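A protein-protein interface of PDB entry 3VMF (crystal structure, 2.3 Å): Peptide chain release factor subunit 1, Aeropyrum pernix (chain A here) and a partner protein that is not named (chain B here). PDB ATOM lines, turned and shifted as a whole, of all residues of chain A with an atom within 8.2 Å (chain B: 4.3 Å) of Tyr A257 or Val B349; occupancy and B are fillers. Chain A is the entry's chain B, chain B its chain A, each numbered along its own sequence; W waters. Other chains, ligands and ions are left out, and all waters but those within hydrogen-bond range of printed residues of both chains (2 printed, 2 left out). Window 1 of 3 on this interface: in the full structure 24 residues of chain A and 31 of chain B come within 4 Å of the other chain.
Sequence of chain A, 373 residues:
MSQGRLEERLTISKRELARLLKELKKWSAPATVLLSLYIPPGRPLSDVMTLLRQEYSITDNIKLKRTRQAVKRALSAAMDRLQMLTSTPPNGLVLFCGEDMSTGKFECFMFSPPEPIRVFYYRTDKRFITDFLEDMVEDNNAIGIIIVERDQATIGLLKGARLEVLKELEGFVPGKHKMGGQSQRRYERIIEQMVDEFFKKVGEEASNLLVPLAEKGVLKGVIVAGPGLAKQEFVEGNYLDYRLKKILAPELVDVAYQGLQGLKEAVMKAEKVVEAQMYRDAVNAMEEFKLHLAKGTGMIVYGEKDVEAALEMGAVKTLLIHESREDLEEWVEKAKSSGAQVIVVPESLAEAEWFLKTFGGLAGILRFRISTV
The side-chain hydroxyl of Tyr A257 is in hydrogen-bond range of the guanidinium group of Arg B416, at 2.9 Å.
A ring nitrogen (NE2) of His B351 lies within hydrogen-bond range of the side-chain hydroxyl (OH) of Tyr A257, at 2.9 Å.
The backbone NH (N) of His B351 sits at hydrogen-bond distance from the backbone carbonyl oxygen (O) of Ala B414 (3.0 Å).
N of Val B349 sits at hydrogen-bond distance from O of Arg B416.
OE1 of Gln A261 lies close to OE1 of Glu A265, 3.1 Å away.
Ala A256 touches Asn B419 (CB to OD1, 3.4 Å).
Tyr A257 touches Val B349.
OD1 of Asn B419 touches CE1 of Tyr A257 (3.6 Å).
CG1 of Val B349 touches CG of Gln A261, 3.5 Å away.
CB of Asn B419 touches OE2 of Glu A265, at 3.6 Å.
Printed residues of chain B within 4 Å of Ala A256: Asn B419.
Printed residues of chain B within 4 Å of Gln A261: Val B349.
Val B349 touches two residues of chain A.
Of the printed residues of chain A, His B351 touches Tyr A257.
Printed residues of chain A within 4 Å of Asn B419: Ala A256, Tyr A257 and Glu A265.
Of the 12 printed residues of chain B, 4 touch a printed residue of chain A.
Printed residues of chain B that touch a printed residue of chain A: Val B349, His B351, Arg B416 and Asn B419.
Hydrophobic or aromatic side chains of chain B that line the printed part of chain A: Val B349 and His B351.
Hydrophobic or aromatic side chains of chain A within 4 Å of the printed part of chain B: Ala A256 and Tyr A257.
Among the printed residues, 7 pairs touch across the chains.
Water W2 lies within hydrogen-bond range of OG of Ser B358 (2.9 Å), N of Gln A261 (3.0 Å) and N of Leu A260 (3.3 Å).
Water W1 bridges the side-chain carboxylate of Glu A265 (3.4 Å) and the side-chain amide nitrogen of Asn B419 (3.4 Å).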
ATOM      1  N   ILE A 147      19.679  -0.635 -14.773  1.00  0.00           N
ATOM      2  CA  ILE A 147      21.030  -0.289 -15.185  1.00  0.00           C
ATOM      3  C   ILE A 147      21.109  -0.184 -16.703  1.00  0.00           C
ATOM      4  O   ILE A 147      20.794  -1.132 -17.433  1.00  0.00           O
ATOM      5  CB  ILE A 147      22.051  -1.316 -14.686  1.00  0.00           C
ATOM      6  CG1 ILE A 147      21.791  -1.625 -13.207  1.00  0.00           C
ATOM      7  CG2 ILE A 147      23.467  -0.796 -14.898  1.00  0.00           C
ATOM      8  CD1 ILE A 147      22.638  -2.730 -12.667  1.00  0.00           C
ATOM      9  N   VAL A 148      21.522   0.982 -17.177  1.00  0.00           N
ATOM     10  CA  VAL A 148      21.466   1.267 -18.602  1.00  0.00           C
ATOM     11  C   VAL A 148      22.857   1.515 -19.147  1.00  0.00           C
ATOM     12  O   VAL A 148      23.653   2.209 -18.528  1.00  0.00           O
ATOM     13  CB  VAL A 148      20.616   2.527 -18.905  1.00  0.00           C
ATOM     14  CG1 VAL A 148      20.342   2.630 -20.393  1.00  0.00           C
ATOM     15  CG2 VAL A 148      19.304   2.477 -18.162  1.00  0.00           C
ATOM     16  N   GLU A 149      23.139   0.909 -20.288  1.00  0.00           N
ATOM     17  CA  GLU A 149      24.314   1.199 -21.089  1.00  0.00           C
ATOM     18  C   GLU A 149      23.802   1.390 -22.485  1.00  0.00           C
ATOM     19  O   GLU A 149      22.630   1.122 -22.757  1.00  0.00           O
ATOM     20  CB  GLU A 149      25.250  -0.002 -21.155  1.00  0.00           C
ATOM     21  CG  GLU A 149      26.220  -0.122 -20.044  1.00  0.00           C
ATOM     22  CD  GLU A 149      27.107  -1.328 -20.235  1.00  0.00           C
ATOM     23  OE1 GLU A 149      27.910  -1.351 -21.205  1.00  0.00           O
ATOM     24  OE2 GLU A 149      26.984  -2.264 -19.435  1.00  0.00           O
ATOM     25  N   GLN A 152      23.359  -2.499 -23.392  1.00  0.00           N
ATOM     26  CA  GLN A 152      22.999  -3.461 -22.370  1.00  0.00           C
ATOM     27  C   GLN A 152      22.095  -2.832 -21.334  1.00  0.00           C
ATOM     28  O   GLN A 152      22.226  -1.659 -21.010  1.00  0.00           O
ATOM     29  CB  GLN A 152      24.250  -3.998 -21.659  1.00  0.00           C
ATOM     30  CG  GLN A 152      24.806  -5.268 -22.248  1.00  0.00           C
ATOM     31  CD  GLN A 152      26.026  -5.783 -21.490  1.00  0.00           C
ATOM     32  OE1 GLN A 152      26.894  -5.010 -21.074  1.00  0.00           O
ATOM     33  NE2 GLN A 152      26.088  -7.092 -21.301  1.00  0.00           N
ATOM     34  N   ALA A 153      21.197  -3.629 -20.785  1.00  0.00           N
ATOM     35  CA  ALA A 153      20.478  -3.182 -19.613  1.00  0.00           C
ATOM     36  C   ALA A 153      20.211  -4.327 -18.659  1.00  0.00           C
ATOM     37  O   ALA A 153      20.167  -5.500 -19.050  1.00  0.00           O
ATOM     38  CB  ALA A 153      19.190  -2.500 -20.004  1.00  0.00           C
ATOM     39  N   THR A 154      20.032  -3.976 -17.397  1.00  0.00           N
ATOM     40  CA  THR A 154      19.660  -4.956 -16.402  1.00  0.00           C
ATOM     41  C   THR A 154      18.551  -4.373 -15.592  1.00  0.00           C
ATOM     42  O   THR A 154      18.664  -3.247 -15.137  1.00  0.00           O
ATOM     43  CB  THR A 154      20.828  -5.291 -15.459  1.00  0.00           C
ATOM     44  OG1 THR A 154      21.843  -5.970 -16.200  1.00  0.00           O
ATOM     45  CG2 THR A 154      20.356  -6.189 -14.322  1.00  0.00           C
ATOM     46  N   ALA A 225      20.747   3.527 -12.905  1.00  0.00           N
ATOM     47  CA  ALA A 225      22.166   3.352 -12.696  1.00  0.00           C
ATOM     48  C   ALA A 225      22.830   3.016 -14.012  1.00  0.00           C
ATOM     49  O   ALA A 225      22.146   2.688 -14.988  1.00  0.00           O
ATOM     50  CB  ALA A 225      22.402   2.228 -11.669  1.00  0.00           C
ATOM     51  N   GLY A 226      24.163   3.091 -14.030  1.00  0.00           N
ATOM     52  CA  GLY A 226      24.955   2.617 -15.152  1.00  0.00           C
ATOM     53  C   GLY A 226      26.179   3.487 -15.380  1.00  0.00           C
ATOM     54  O   GLY A 226      26.409   4.449 -14.660  1.00  0.00           O
ATOM     55  N   PRO A 227      26.986   3.148 -16.382  1.00  0.00           N
ATOM     56  CA  PRO A 227      28.213   3.915 -16.586  1.00  0.00           C
ATOM     57  C   PRO A 227      28.022   5.069 -17.554  1.00  0.00           C
ATOM     58  O   PRO A 227      27.361   4.934 -18.594  1.00  0.00           O
ATOM     59  CB  PRO A 227      29.181   2.875 -17.156  1.00  0.00           C
ATOM     60  CG  PRO A 227      28.301   1.897 -17.876  1.00  0.00           C
ATOM     61  CD  PRO A 227      26.915   1.963 -17.257  1.00  0.00           C
ATOM     62  N   ASP A 254      26.452   6.067 -10.886  1.00  0.00           N
ATOM     63  CA  ASP A 254      27.420   5.479 -11.803  1.00  0.00           C
ATOM     64  C   ASP A 254      27.916   4.122 -11.321  1.00  0.00           C
ATOM     65  O   ASP A 254      28.466   4.017 -10.232  1.00  0.00           O
ATOM     66  CB  ASP A 254      28.612   6.393 -12.024  1.00  0.00           C
ATOM     67  CG  ASP A 254      29.429   5.964 -13.222  1.00  0.00           C
ATOM     68  OD1 ASP A 254      30.166   4.978 -13.083  1.00  0.00           O
ATOM     69  OD2 ASP A 254      29.304   6.575 -14.308  1.00  0.00           O
ATOM     70  N   VAL A 255      27.701   3.085 -12.131  1.00  0.00           N
ATOM     71  CA  VAL A 255      28.286   1.763 -11.880  1.00  0.00           C
ATOM     72  C   VAL A 255      28.852   1.219 -13.196  1.00  0.00           C
ATOM     73  O   VAL A 255      28.379   1.570 -14.280  1.00  0.00           O
ATOM     74  CB  VAL A 255      27.269   0.722 -11.325  1.00  0.00           C
ATOM     75  CG1 VAL A 255      26.504   1.262 -10.139  1.00  0.00           C
ATOM     76  CG2 VAL A 255      26.320   0.299 -12.404  1.00  0.00           C
ATOM     77  N   ALA A 256      29.848   0.342 -13.106  1.00  0.00           N
ATOM     78  CA  ALA A 256      30.472  -0.185 -14.305  1.00  0.00           C
ATOM     79  C   ALA A 256      29.812  -1.456 -14.899  1.00  0.00           C
ATOM     80  O   ALA A 256      29.867  -1.666 -16.089  1.00  0.00           O
ATOM     81  CB  ALA A 256      31.965  -0.401 -14.064  1.00  0.00           C
ATOM     82  N   TYR A 257      29.186  -2.282 -14.077  1.00  0.00           N
ATOM     83  CA  TYR A 257      28.787  -3.611 -14.511  1.00  0.00           C
ATOM     84  C   TYR A 257      27.296  -3.766 -14.638  1.00  0.00           C
ATOM     85  O   TYR A 257      26.523  -2.982 -14.062  1.00  0.00           O
ATOM     86  CB  TYR A 257      29.261  -4.668 -13.503  1.00  0.00           C
ATOM     87  CG  TYR A 257      30.748  -4.928 -13.500  1.00  0.00           C
ATOM     88  CD1 TYR A 257      31.595  -4.207 -12.671  1.00  0.00           C
ATOM     89  CD2 TYR A 257      31.307  -5.920 -14.306  1.00  0.00           C
ATOM     90  CE1 TYR A 257      32.966  -4.453 -12.651  1.00  0.00           C
ATOM     91  CE2 TYR A 257      32.678  -6.171 -14.289  1.00  0.00           C
ATOM     92  CZ  TYR A 257      33.502  -5.434 -13.462  1.00  0.00           C
ATOM     93  OH  TYR A 257      34.871  -5.677 -13.439  1.00  0.00           O
ATOM     94  N   GLN A 258      26.910  -4.809 -15.370  1.00  0.00           N
ATOM     95  CA  GLN A 258      25.520  -5.242 -15.479  1.00  0.00           C
ATOM     96  C   GLN A 258      25.209  -6.362 -14.491  1.00  0.00           C
ATOM     97  O   GLN A 258      26.056  -6.726 -13.658  1.00  0.00           O
ATOM     98  CB  GLN A 258      25.213  -5.699 -16.906  1.00  0.00           C
ATOM     99  CG  GLN A 258      25.350  -4.592 -17.938  1.00  0.00           C
ATOM    100  CD  GLN A 258      24.192  -3.601 -17.885  1.00  0.00           C
ATOM    101  OE1 GLN A 258      23.044  -3.986 -17.647  1.00  0.00           O
ATOM    102  NE2 GLN A 258      24.487  -2.321 -18.107  1.00  0.00           N
ATOM    103  N   GLY A 259      23.993  -6.900 -14.575  1.00  0.00           N
ATOM    104  CA  GLY A 259      23.587  -8.028 -13.747  1.00  0.00           C
ATOM    105  C   GLY A 259      23.628  -7.773 -12.251  1.00  0.00           C
ATOM    106  O   GLY A 259      23.537  -6.626 -11.795  1.00  0.00           O
ATOM    107  N   LEU A 260      23.776  -8.840 -11.472  1.00  0.00           N
ATOM    108  CA  LEU A 260      23.704  -8.714 -10.013  1.00  0.00           C
ATOM    109  C   LEU A 260      24.858  -7.895  -9.449  1.00  0.00           C
ATOM    110  O   LEU A 260      24.668  -7.097  -8.520  1.00  0.00           O
ATOM    111  CB  LEU A 260      23.642 -10.083  -9.343  1.00  0.00           C
ATOM    112  CG  LEU A 260      23.447 -10.034  -7.830  1.00  0.00           C
ATOM    113  CD1 LEU A 260      22.212  -9.236  -7.520  1.00  0.00           C
ATOM    114  CD2 LEU A 260      23.305 -11.437  -7.276  1.00  0.00           C
ATOM    115  N   GLN A 261      26.047  -8.095 -10.016  1.00  0.00           N
ATOM    116  CA  GLN A 261      27.190  -7.256  -9.702  1.00  0.00           C
ATOM    117  C   GLN A 261      26.826  -5.773  -9.828  1.00  0.00           C
ATOM    118  O   GLN A 261      27.088  -4.966  -8.918  1.00  0.00           O
ATOM    119  CB  GLN A 261      28.344  -7.577 -10.648  1.00  0.00           C
ATOM    120  CG  GLN A 261      29.690  -7.582  -9.963  1.00  0.00           C
ATOM    121  CD  GLN A 261      30.065  -6.240  -9.420  1.00  0.00           C
ATOM    122  OE1 GLN A 261      29.817  -5.217 -10.059  1.00  0.00           O
ATOM    123  NE2 GLN A 261      30.664  -6.219  -8.233  1.00  0.00           N
ATOM    124  N   GLY A 262      26.216  -5.428 -10.962  1.00  0.00           N
ATOM    125  CA  GLY A 262      25.767  -4.074 -11.194  1.00  0.00           C
ATOM    126  C   GLY A 262      24.742  -3.617 -10.177  1.00  0.00           C
ATOM    127  O   GLY A 262      24.851  -2.516  -9.632  1.00  0.00           O
ATOM    128  N   LEU A 263      23.752  -4.459  -9.908  1.00  0.00           N
ATOM    129  CA  LEU A 263      22.725  -4.125  -8.905  1.00  0.00           C
ATOM    130  C   LEU A 263      23.314  -3.870  -7.510  1.00  0.00           C
ATOM    131  O   LEU A 263      22.943  -2.910  -6.856  1.00  0.00           O
ATOM    132  CB  LEU A 263      21.662  -5.210  -8.819  1.00  0.00           C
ATOM    133  CG  LEU A 263      20.990  -5.585 -10.131  1.00  0.00           C
ATOM    134  CD1 LEU A 263      20.090  -6.772  -9.909  1.00  0.00           C
ATOM    135  CD2 LEU A 263      20.201  -4.397 -10.711  1.00  0.00           C
ATOM    136  N   LYS A 264      24.246  -4.718  -7.071  1.00  0.00           N
ATOM    137  CA  LYS A 264      24.854  -4.541  -5.763  1.00  0.00           C
ATOM    138  C   LYS A 264      25.581  -3.211  -5.704  1.00  0.00           C
ATOM    139  O   LYS A 264      25.375  -2.425  -4.773  1.00  0.00           O
ATOM    140  CB  LYS A 264      25.837  -5.667  -5.473  1.00  0.00           C
ATOM    141  CG  LYS A 264      25.208  -7.045  -5.383  1.00  0.00           C
ATOM    142  CD  LYS A 264      26.244  -8.145  -5.703  1.00  0.00           C
ATOM    143  CE  LYS A 264      25.805  -9.488  -5.136  1.00  0.00           C
ATOM    144  NZ  LYS A 264      26.657 -10.620  -5.598  1.00  0.00           N
ATOM    145  N   GLU A 265      26.444  -2.988  -6.695  1.00  0.00           N
ATOM    146  CA  GLU A 265      27.125  -1.711  -6.869  1.00  0.00           C
ATOM    147  C   GLU A 265      26.143  -0.539  -6.713  1.00  0.00           C
ATOM    148  O   GLU A 265      26.350   0.346  -5.878  1.00  0.00           O
ATOM    149  CB  GLU A 265      27.817  -1.660  -8.238  1.00  0.00           C
ATOM    150  CG  GLU A 265      29.342  -1.719  -8.216  1.00  0.00           C
ATOM    151  CD  GLU A 265      29.971  -1.406  -9.593  1.00  0.00           C
ATOM    152  OE1 GLU A 265      29.682  -2.153 -10.566  1.00  0.00           O
ATOM    153  OE2 GLU A 265      30.737  -0.405  -9.706  1.00  0.00           O
ATOM    154  N   ALA A 266      25.053  -0.554  -7.478  1.00  0.00           N
ATOM    155  CA  ALA A 266      24.061   0.546  -7.420  1.00  0.00           C
ATOM    156  C   ALA A 266      23.415   0.733  -6.038  1.00  0.00           C
ATOM    157  O   ALA A 266      23.339   1.848  -5.529  1.00  0.00           O
ATOM    158  CB  ALA A 266      22.990   0.376  -8.492  1.00  0.00           C
ATOM    159  N   LYS B 102      37.016  -3.289 -17.629  1.00  0.00           N
ATOM    160  CA  LYS B 102      36.558  -4.520 -18.261  1.00  0.00           C
ATOM    161  C   LYS B 102      36.876  -4.552 -19.765  1.00  0.00           C
ATOM    162  O   LYS B 102      37.156  -5.612 -20.322  1.00  0.00           O
ATOM    163  CB  LYS B 102      35.071  -4.801 -17.984  1.00  0.00           C
ATOM    164  CG  LYS B 102      34.103  -3.680 -18.341  1.00  0.00           C
ATOM    165  CD  LYS B 102      32.680  -3.983 -17.862  1.00  0.00           C
ATOM    166  CE  LYS B 102      31.922  -4.805 -18.893  1.00  0.00           C
ATOM    167  NZ  LYS B 102      31.634  -6.199 -18.435  1.00  0.00           N
ATOM    168  N   PRO B 348      32.820 -12.640  -6.993  1.00  0.00           N
ATOM    169  CA  PRO B 348      33.366 -11.541  -7.791  1.00  0.00           C
ATOM    170  C   PRO B 348      33.073 -11.842  -9.268  1.00  0.00           C
ATOM    171  O   PRO B 348      32.663 -12.970  -9.572  1.00  0.00           O
ATOM    172  CB  PRO B 348      34.868 -11.696  -7.544  1.00  0.00           C
ATOM    173  CG  PRO B 348      35.039 -13.226  -7.521  1.00  0.00           C
ATOM    174  CD  PRO B 348      33.805 -13.728  -6.799  1.00  0.00           C
ATOM    175  N   VAL B 349      33.274 -10.897 -10.184  1.00  0.00           N
ATOM    176  CA  VAL B 349      33.235 -11.307 -11.588  1.00  0.00           C
ATOM    177  C   VAL B 349      34.604 -11.836 -12.057  1.00  0.00           C
ATOM    178  O   VAL B 349      35.665 -11.317 -11.685  1.00  0.00           O
ATOM    179  CB  VAL B 349      32.528 -10.288 -12.591  1.00  0.00           C
ATOM    180  CG1 VAL B 349      32.237  -8.956 -11.948  1.00  0.00           C
ATOM    181  CG2 VAL B 349      33.275 -10.144 -13.909  1.00  0.00           C
ATOM    182  N   ILE B 350      34.547 -12.917 -12.823  1.00  0.00           N
ATOM    183  CA  ILE B 350      35.716 -13.521 -13.391  1.00  0.00           C
ATOM    184  C   ILE B 350      35.918 -12.946 -14.782  1.00  0.00           C
ATOM    185  O   ILE B 350      35.076 -13.142 -15.647  1.00  0.00           O
ATOM    186  CB  ILE B 350      35.554 -15.075 -13.482  1.00  0.00           C
ATOM    187  CG1 ILE B 350      35.256 -15.657 -12.107  1.00  0.00           C
ATOM    188  CG2 ILE B 350      36.812 -15.736 -14.031  1.00  0.00           C
ATOM    189  CD1 ILE B 350      36.207 -15.179 -11.023  1.00  0.00           C
ATOM    190  N   HIS B 351      37.034 -12.245 -14.985  1.00  0.00           N
ATOM    191  CA  HIS B 351      37.470 -11.829 -16.315  1.00  0.00           C
ATOM    192  C   HIS B 351      38.471 -12.833 -16.894  1.00  0.00           C
ATOM    193  O   HIS B 351      39.637 -12.858 -16.489  1.00  0.00           O
ATOM    194  CB  HIS B 351      38.082 -10.421 -16.282  1.00  0.00           C
ATOM    195  CG  HIS B 351      37.101  -9.350 -15.918  1.00  0.00           C
ATOM    196  ND1 HIS B 351      36.675  -8.392 -16.813  1.00  0.00           N
ATOM    197  CD2 HIS B 351      36.444  -9.097 -14.759  1.00  0.00           C
ATOM    198  CE1 HIS B 351      35.801  -7.599 -16.220  1.00  0.00           C
ATOM    199  NE2 HIS B 351      35.651  -7.999 -14.973  1.00  0.00           N
ATOM    200  N   SER B 356      33.390 -12.157 -19.033  1.00  0.00           N
ATOM    201  CA  SER B 356      33.319 -11.658 -17.666  1.00  0.00           C
ATOM    202  C   SER B 356      32.016 -12.076 -17.015  1.00  0.00           C
ATOM    203  O   SER B 356      30.974 -11.495 -17.260  1.00  0.00           O
ATOM    204  CB  SER B 356      33.505 -10.139 -17.580  1.00  0.00           C
ATOM    205  OG  SER B 356      32.517  -9.440 -18.292  1.00  0.00           O
ATOM    206  N   VAL B 357      32.091 -13.094 -16.170  1.00  0.00           N
ATOM    207  CA  VAL B 357      30.900 -13.715 -15.620  1.00  0.00           C
ATOM    208  C   VAL B 357      31.079 -13.895 -14.136  1.00  0.00           C
ATOM    209  O   VAL B 357      32.083 -14.469 -13.712  1.00  0.00           O
ATOM    210  CB  VAL B 357      30.708 -15.125 -16.203  1.00  0.00           C
ATOM    211  CG1 VAL B 357      29.525 -15.805 -15.545  1.00  0.00           C
ATOM    212  CG2 VAL B 357      30.557 -15.069 -17.710  1.00  0.00           C
ATOM    213  N   SER B 358      30.121 -13.427 -13.342  1.00  0.00           N
ATOM    214  CA  SER B 358      30.201 -13.679 -11.909  1.00  0.00           C
ATOM    215  C   SER B 358      30.277 -15.189 -11.646  1.00  0.00           C
ATOM    216  O   SER B 358      29.645 -15.981 -12.360  1.00  0.00           O
ATOM    217  CB  SER B 358      29.036 -13.060 -11.154  1.00  0.00           C
ATOM    218  OG  SER B 358      29.132 -11.658 -11.187  1.00  0.00           O
ATOM    219  N   ALA B 414      41.242 -12.634 -13.896  1.00  0.00           N
ATOM    220  CA  ALA B 414      41.189 -11.707 -12.773  1.00  0.00           C
ATOM    221  C   ALA B 414      39.844 -11.810 -12.074  1.00  0.00           C
ATOM    222  O   ALA B 414      38.856 -12.235 -12.649  1.00  0.00           O
ATOM    223  CB  ALA B 414      41.433 -10.293 -13.233  1.00  0.00           C
ATOM    224  N   MET B 415      39.828 -11.447 -10.809  1.00  0.00           N
ATOM    225  CA  MET B 415      38.606 -11.448 -10.047  1.00  0.00           C
ATOM    226  C   MET B 415      38.404  -9.993  -9.694  1.00  0.00           C
ATOM    227  O   MET B 415      39.336  -9.330  -9.202  1.00  0.00           O
ATOM    228  CB  MET B 415      38.755 -12.283  -8.765  1.00  0.00           C
ATOM    229  CG  MET B 415      39.243 -13.720  -8.945  1.00  0.00           C
ATOM    230  SD  MET B 415      39.822 -14.535  -7.390  1.00  0.00           S
ATOM    231  CE  MET B 415      38.625 -13.987  -6.195  1.00  0.00           C
ATOM    232  N   ARG B 416      37.214  -9.473  -9.987  1.00  0.00           N
ATOM    233  CA  ARG B 416      36.917  -8.083  -9.659  1.00  0.00           C
ATOM    234  C   ARG B 416      35.585  -7.970  -8.965  1.00  0.00           C
ATOM    235  O   ARG B 416      34.685  -8.758  -9.200  1.00  0.00           O
ATOM    236  CB  ARG B 416      36.980  -7.192 -10.885  1.00  0.00           C
ATOM    237  CG  ARG B 416      38.246  -7.347 -11.635  1.00  0.00           C
ATOM    238  CD  ARG B 416      38.475  -6.284 -12.680  1.00  0.00           C
ATOM    239  NE  ARG B 416      38.906  -5.041 -12.066  1.00  0.00           N
ATOM    240  CZ  ARG B 416      38.209  -3.910 -12.096  1.00  0.00           C
ATOM    241  NH1 ARG B 416      37.032  -3.856 -12.722  1.00  0.00           N
ATOM    242  NH2 ARG B 416      38.696  -2.827 -11.514  1.00  0.00           N
ATOM    243  N   ASN B 419      34.015  -2.772  -8.503  1.00  0.00           N
ATOM    244  CA  ASN B 419      34.922  -2.046  -9.389  1.00  0.00           C
ATOM    245  C   ASN B 419      36.369  -1.905  -8.898  1.00  0.00           C
ATOM    246  O   ASN B 419      36.995  -0.834  -8.983  1.00  0.00           O
ATOM    247  CB  ASN B 419      34.332  -0.686  -9.778  1.00  0.00           C
ATOM    248  CG  ASN B 419      34.507  -0.387 -11.251  1.00  0.00           C
ATOM    249  OD1 ASN B 419      34.558  -1.306 -12.097  1.00  0.00           O
ATOM    250  ND2 ASN B 419      34.626   0.898 -11.573  1.00  0.00           N
HETATM  251  O   HOH W   1      31.700   2.597 -10.965  1.00  0.00           O
HETATM  252  O   HOH W   2      26.739 -10.178 -11.996  1.00  0.00           O
